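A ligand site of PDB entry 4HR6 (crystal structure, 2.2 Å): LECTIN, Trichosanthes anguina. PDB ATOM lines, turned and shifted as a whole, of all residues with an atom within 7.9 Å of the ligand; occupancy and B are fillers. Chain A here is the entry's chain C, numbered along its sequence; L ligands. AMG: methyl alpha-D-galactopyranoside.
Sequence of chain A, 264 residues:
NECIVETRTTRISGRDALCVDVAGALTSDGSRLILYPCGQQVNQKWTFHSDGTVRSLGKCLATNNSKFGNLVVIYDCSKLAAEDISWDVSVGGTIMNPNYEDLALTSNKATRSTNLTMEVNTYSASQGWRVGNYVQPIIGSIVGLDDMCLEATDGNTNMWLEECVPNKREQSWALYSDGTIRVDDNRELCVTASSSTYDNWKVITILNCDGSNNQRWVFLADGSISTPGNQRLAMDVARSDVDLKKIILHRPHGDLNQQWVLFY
O of Val 22 touches O4 of the ligand, at 3.8 Å.
C of Ala 23 touches O4 of the ligand, at 3.98 Å.
CD1 of Ile 34 touches C6 of the ligand, 3.98 Å away.
Tyr 36 touches the ligand (OH to O1, 3.7 Å).
The side-chain carboxylate of Asp 21 sits at hydrogen-bond distance from the side-chain amide nitrogen of Asn 43, at 3.1 Å.
O of Asp 21 sits at hydrogen-bond distance from N of Ile 34 (2.7 Å).
OD1 of Asp 21 lies within hydrogen-bond range of NE2 of Gln 44.
O of Asn 43 sits at hydrogen-bond distance from N of Val 22 (3.2 Å).
The backbone carbonyl oxygen (O) of Arg 32 lies within hydrogen-bond range of the backbone NH (N) of Ala 23, 2.8 Å away.
The side-chain carboxylate (OD1) of Asp 21 lies within hydrogen-bond range of an oxygen (O3) of the ligand.
An oxygen (O3) of the ligand lies within hydrogen-bond range of the side-chain amide nitrogen (ND2) of Asn 43, 2.8 Å away.
The backbone NH (N) of Gly 24 lies within hydrogen-bond range of an oxygen (O4) of the ligand (3.0 Å).
NE2 of Gln 41 is in hydrogen-bond range of O3 of the ligand (3.1 Å).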
ATOM      1  N   VAL A  20      15.019 -13.430   2.846  1.00  0.00           N
ATOM      2  CA  VAL A  20      15.078 -13.094   1.439  1.00  0.00           C
ATOM      3  C   VAL A  20      13.903 -13.788   0.720  1.00  0.00           C
ATOM      4  O   VAL A  20      13.674 -14.992   0.861  1.00  0.00           O
ATOM      5  CB  VAL A  20      16.446 -13.490   0.846  1.00  0.00           C
ATOM      6  CG1 VAL A  20      16.483 -13.256  -0.654  1.00  0.00           C
ATOM      7  CG2 VAL A  20      17.552 -12.708   1.540  1.00  0.00           C
ATOM      8  N   ASP A  21      13.161 -12.985  -0.026  1.00  0.00           N
ATOM      9  CA  ASP A  21      11.816 -13.350  -0.478  1.00  0.00           C
ATOM     10  C   ASP A  21      11.594 -12.678  -1.834  1.00  0.00           C
ATOM     11  O   ASP A  21      11.766 -11.460  -1.956  1.00  0.00           O
ATOM     12  CB  ASP A  21      10.802 -12.894   0.591  1.00  0.00           C
ATOM     13  CG  ASP A  21       9.342 -13.028   0.147  1.00  0.00           C
ATOM     14  OD1 ASP A  21       8.504 -13.515   0.941  1.00  0.00           O
ATOM     15  OD2 ASP A  21       9.029 -12.628  -0.996  1.00  0.00           O
ATOM     16  N   VAL A  22      11.265 -13.462  -2.856  1.00  0.00           N
ATOM     17  CA  VAL A  22      11.016 -12.889  -4.177  1.00  0.00           C
ATOM     18  C   VAL A  22       9.592 -12.321  -4.177  1.00  0.00           C
ATOM     19  O   VAL A  22       8.619 -13.044  -3.955  1.00  0.00           O
ATOM     20  CB  VAL A  22      11.332 -13.854  -5.371  1.00  0.00           C
ATOM     21  CG1 VAL A  22      10.948 -15.289  -5.064  1.00  0.00           C
ATOM     22  CG2 VAL A  22      10.667 -13.374  -6.652  1.00  0.00           C
ATOM     23  N   ALA A  23       9.490 -11.004  -4.406  1.00  0.00           N
ATOM     24  CA  ALA A  23       8.262 -10.247  -4.158  1.00  0.00           C
ATOM     25  C   ALA A  23       7.013 -10.850  -4.811  1.00  0.00           C
ATOM     26  O   ALA A  23       6.967 -11.005  -6.036  1.00  0.00           O
ATOM     27  CB  ALA A  23       8.449  -8.803  -4.623  1.00  0.00           C
ATOM     28  N   GLY A  24       6.032 -11.222  -3.989  1.00  0.00           N
ATOM     29  CA  GLY A  24       4.720 -11.681  -4.447  1.00  0.00           C
ATOM     30  C   GLY A  24       4.646 -13.029  -5.166  1.00  0.00           C
ATOM     31  O   GLY A  24       3.582 -13.421  -5.643  1.00  0.00           O
ATOM     32  N   ALA A  25       5.780 -13.736  -5.242  1.00  0.00           N
ATOM     33  CA  ALA A  25       5.875 -15.013  -5.946  1.00  0.00           C
ATOM     34  C   ALA A  25       5.876 -14.838  -7.468  1.00  0.00           C
ATOM     35  O   ALA A  25       5.550 -15.779  -8.194  1.00  0.00           O
ATOM     36  CB  ALA A  25       4.781 -15.979  -5.501  1.00  0.00           C
ATOM     37  N   LEU A  26       6.248 -13.648  -7.941  1.00  0.00           N
ATOM     38  CA  LEU A  26       6.362 -13.355  -9.365  1.00  0.00           C
ATOM     39  C   LEU A  26       7.489 -14.152  -9.980  1.00  0.00           C
ATOM     40  O   LEU A  26       8.494 -14.396  -9.315  1.00  0.00           O
ATOM     41  CB  LEU A  26       6.634 -11.859  -9.607  1.00  0.00           C
ATOM     42  CG  LEU A  26       5.446 -10.896  -9.702  1.00  0.00           C
ATOM     43  CD1 LEU A  26       4.577 -10.892  -8.455  1.00  0.00           C
ATOM     44  CD2 LEU A  26       5.971  -9.489  -9.996  1.00  0.00           C
ATOM     45  N   ARG A  32      11.692  -8.681  -8.510  1.00  0.00           N
ATOM     46  CA  ARG A  32      12.524  -8.108  -7.440  1.00  0.00           C
ATOM     47  C   ARG A  32      12.436  -8.939  -6.152  1.00  0.00           C
ATOM     48  O   ARG A  32      11.442  -9.643  -5.916  1.00  0.00           O
ATOM     49  CB  ARG A  32      12.117  -6.660  -7.183  1.00  0.00           C
ATOM     50  N   ILE A  34      12.774  -8.954  -1.860  1.00  0.00           N
ATOM     51  CA  ILE A  34      12.624  -8.153  -0.656  1.00  0.00           C
ATOM     52  C   ILE A  34      13.060  -8.897   0.609  1.00  0.00           C
ATOM     53  O   ILE A  34      13.266 -10.115   0.568  1.00  0.00           O
ATOM     54  CB  ILE A  34      11.148  -7.722  -0.461  1.00  0.00           C
ATOM     55  CG1 ILE A  34      10.226  -8.953  -0.451  1.00  0.00           C
ATOM     56  CG2 ILE A  34      10.725  -6.767  -1.575  1.00  0.00           C
ATOM     57  CD1 ILE A  34       8.842  -8.688   0.115  1.00  0.00           C
ATOM     58  N   LEU A  35      13.177  -8.176   1.720  1.00  0.00           N
ATOM     59  CA  LEU A  35      13.128  -8.767   3.045  1.00  0.00           C
ATOM     60  C   LEU A  35      11.663  -8.935   3.410  1.00  0.00           C
ATOM     61  O   LEU A  35      10.864  -8.046   3.156  1.00  0.00           O
ATOM     62  CB  LEU A  35      13.751  -7.855   4.097  1.00  0.00           C
ATOM     63  CG  LEU A  35      15.257  -7.611   4.111  1.00  0.00           C
ATOM     64  CD1 LEU A  35      15.581  -6.826   5.373  1.00  0.00           C
ATOM     65  CD2 LEU A  35      16.052  -8.917   4.054  1.00  0.00           C
ATOM     66  N   TYR A  36      11.323 -10.051   4.055  1.00  0.00           N
ATOM     67  CA  TYR A  36       9.953 -10.314   4.466  1.00  0.00           C
ATOM     68  C   TYR A  36       9.951 -11.299   5.642  1.00  0.00           C
ATOM     69  O   TYR A  36      10.835 -12.140   5.722  1.00  0.00           O
ATOM     70  CB  TYR A  36       9.150 -10.875   3.281  1.00  0.00           C
ATOM     71  CG  TYR A  36       7.646 -10.717   3.414  1.00  0.00           C
ATOM     72  CD1 TYR A  36       7.002  -9.545   3.023  1.00  0.00           C
ATOM     73  CD2 TYR A  36       6.866 -11.739   3.949  1.00  0.00           C
ATOM     74  CE1 TYR A  36       5.624  -9.388   3.151  1.00  0.00           C
ATOM     75  CE2 TYR A  36       5.490 -11.605   4.085  1.00  0.00           C
ATOM     76  CZ  TYR A  36       4.878 -10.428   3.675  1.00  0.00           C
ATOM     77  OH  TYR A  36       3.516 -10.292   3.814  1.00  0.00           O
ATOM     78  N   PRO A  37       8.974 -11.208   6.556  1.00  0.00           N
ATOM     79  CA  PRO A  37       8.859 -12.205   7.613  1.00  0.00           C
ATOM     80  C   PRO A  37       9.098 -13.631   7.121  1.00  0.00           C
ATOM     81  O   PRO A  37       8.541 -14.027   6.093  1.00  0.00           O
ATOM     82  CB  PRO A  37       7.414 -12.031   8.092  1.00  0.00           C
ATOM     83  CG  PRO A  37       7.102 -10.598   7.825  1.00  0.00           C
ATOM     84  CD  PRO A  37       8.046 -10.081   6.770  1.00  0.00           C
ATOM     85  N   GLY A  39       8.806 -17.474   6.622  1.00  0.00           N
ATOM     86  CA  GLY A  39       7.747 -18.467   6.668  1.00  0.00           C
ATOM     87  C   GLY A  39       8.104 -19.630   5.767  1.00  0.00           C
ATOM     88  O   GLY A  39       9.199 -19.695   5.222  1.00  0.00           O
ATOM     89  N   GLN A  41       6.811 -20.403   2.852  1.00  0.00           N
ATOM     90  CA  GLN A  41       6.365 -20.192   1.477  1.00  0.00           C
ATOM     91  C   GLN A  41       7.480 -20.415   0.470  1.00  0.00           C
ATOM     92  O   GLN A  41       8.615 -19.988   0.675  1.00  0.00           O
ATOM     93  CB  GLN A  41       5.726 -18.801   1.269  1.00  0.00           C
ATOM     94  CG  GLN A  41       6.536 -17.604   1.769  1.00  0.00           C
ATOM     95  CD  GLN A  41       6.029 -17.092   3.106  1.00  0.00           C
ATOM     96  OE1 GLN A  41       5.858 -17.856   4.060  1.00  0.00           O
ATOM     97  NE2 GLN A  41       5.767 -15.797   3.178  1.00  0.00           N
ATOM     98  N   VAL A  42       7.123 -21.056  -0.646  1.00  0.00           N
ATOM     99  CA  VAL A  42       8.082 -21.517  -1.659  1.00  0.00           C
ATOM    100  C   VAL A  42       8.928 -20.405  -2.272  1.00  0.00           C
ATOM    101  O   VAL A  42      10.021 -20.658  -2.786  1.00  0.00           O
ATOM    102  CB  VAL A  42       7.349 -22.301  -2.784  1.00  0.00           C
ATOM    103  CG1 VAL A  42       6.512 -21.354  -3.653  1.00  0.00           C
ATOM    104  CG2 VAL A  42       8.339 -23.082  -3.637  1.00  0.00           C
ATOM    105  N   ASN A  43       8.432 -19.168  -2.223  1.00  0.00           N
ATOM    106  CA  ASN A  43       9.193 -17.997  -2.721  1.00  0.00           C
ATOM    107  C   ASN A  43      10.281 -17.529  -1.739  1.00  0.00           C
ATOM    108  O   ASN A  43      11.006 -16.568  -2.022  1.00  0.00           O
ATOM    109  CB  ASN A  43       8.257 -16.831  -3.111  1.00  0.00           C
ATOM    110  CG  ASN A  43       7.331 -16.401  -1.981  1.00  0.00           C
ATOM    111  OD1 ASN A  43       6.596 -17.211  -1.417  1.00  0.00           O
ATOM    112  ND2 ASN A  43       7.364 -15.111  -1.664  1.00  0.00           N
ATOM    113  N   GLN A  44      10.386 -18.212  -0.590  1.00  0.00           N
ATOM    114  CA  GLN A  44      11.507 -17.996   0.339  1.00  0.00           C
ATOM    115  C   GLN A  44      12.517 -19.148   0.353  1.00  0.00           C
ATOM    116  O   GLN A  44      13.533 -19.056   1.038  1.00  0.00           O
ATOM    117  CB  GLN A  44      10.982 -17.734   1.759  1.00  0.00           C
ATOM    118  CG  GLN A  44      10.461 -16.323   1.928  1.00  0.00           C
ATOM    119  CD  GLN A  44       9.953 -16.029   3.311  1.00  0.00           C
ATOM    120  OE1 GLN A  44      10.091 -16.849   4.232  1.00  0.00           O
ATOM    121  NE2 GLN A  44       9.343 -14.862   3.476  1.00  0.00           N
ATOM    122  N   ARG A 112      10.076  -4.346   6.674  1.00  0.00           N
ATOM    123  CA  ARG A 112       9.326  -5.273   5.829  1.00  0.00           C
ATOM    124  C   ARG A 112       9.162  -4.718   4.399  1.00  0.00           C
ATOM    125  O   ARG A 112       8.890  -3.537   4.218  1.00  0.00           O
ATOM    126  CB  ARG A 112       7.964  -5.533   6.484  1.00  0.00           C
ATOM    127  CG  ARG A 112       6.915  -6.184   5.580  1.00  0.00           C
ATOM    128  CD  ARG A 112       5.521  -6.085   6.193  1.00  0.00           C
ATOM    129  NE  ARG A 112       5.350  -7.005   7.319  1.00  0.00           N
ATOM    130  CZ  ARG A 112       4.424  -6.883   8.274  1.00  0.00           C
ATOM    131  NH1 ARG A 112       3.597  -5.845   8.286  1.00  0.00           N
ATOM    132  NH2 ARG A 112       4.358  -7.793   9.237  1.00  0.00           N
ATOM    133  N   SER A 113       9.337  -5.583   3.412  1.00  0.00           N
ATOM    134  CA  SER A 113       9.180  -5.250   1.988  1.00  0.00           C
ATOM    135  C   SER A 113      10.238  -4.294   1.407  1.00  0.00           C
ATOM    136  O   SER A 113      10.017  -3.698   0.359  1.00  0.00           O
ATOM    137  CB  SER A 113       7.758  -4.729   1.698  1.00  0.00           C
ATOM    138  OG  SER A 113       6.760  -5.574   2.255  1.00  0.00           O
HETATM  139  C1  AMG L   1       2.762 -12.406  -0.355  1.00  0.00           C
HETATM  140  C2  AMG L   1       3.773 -13.548  -0.208  1.00  0.00           C
HETATM  141  C3  AMG L   1       4.997 -13.117   0.602  1.00  0.00           C
HETATM  142  C4  AMG L   1       5.579 -11.785   0.129  1.00  0.00           C
HETATM  143  C5  AMG L   1       4.494 -10.730  -0.117  1.00  0.00           C
HETATM  144  C6  AMG L   1       5.059  -9.496  -0.820  1.00  0.00           C
HETATM  145  C7  AMG L   1       0.746 -12.173   0.940  1.00  0.00           C
HETATM  146  O1  AMG L   1       2.184 -12.093   0.924  1.00  0.00           O
HETATM  147  O2  AMG L   1       3.138 -14.653   0.439  1.00  0.00           O
HETATM  148  O3  AMG L   1       6.015 -14.131   0.533  1.00  0.00           O
HETATM  149  O4  AMG L   1       6.354 -11.994  -1.057  1.00  0.00           O
HETATM  150  O5  AMG L   1       3.414 -11.253  -0.913  1.00  0.00           O
HETATM  151  O6  AMG L   1       4.428  -8.304  -0.321  1.00  0.00           O
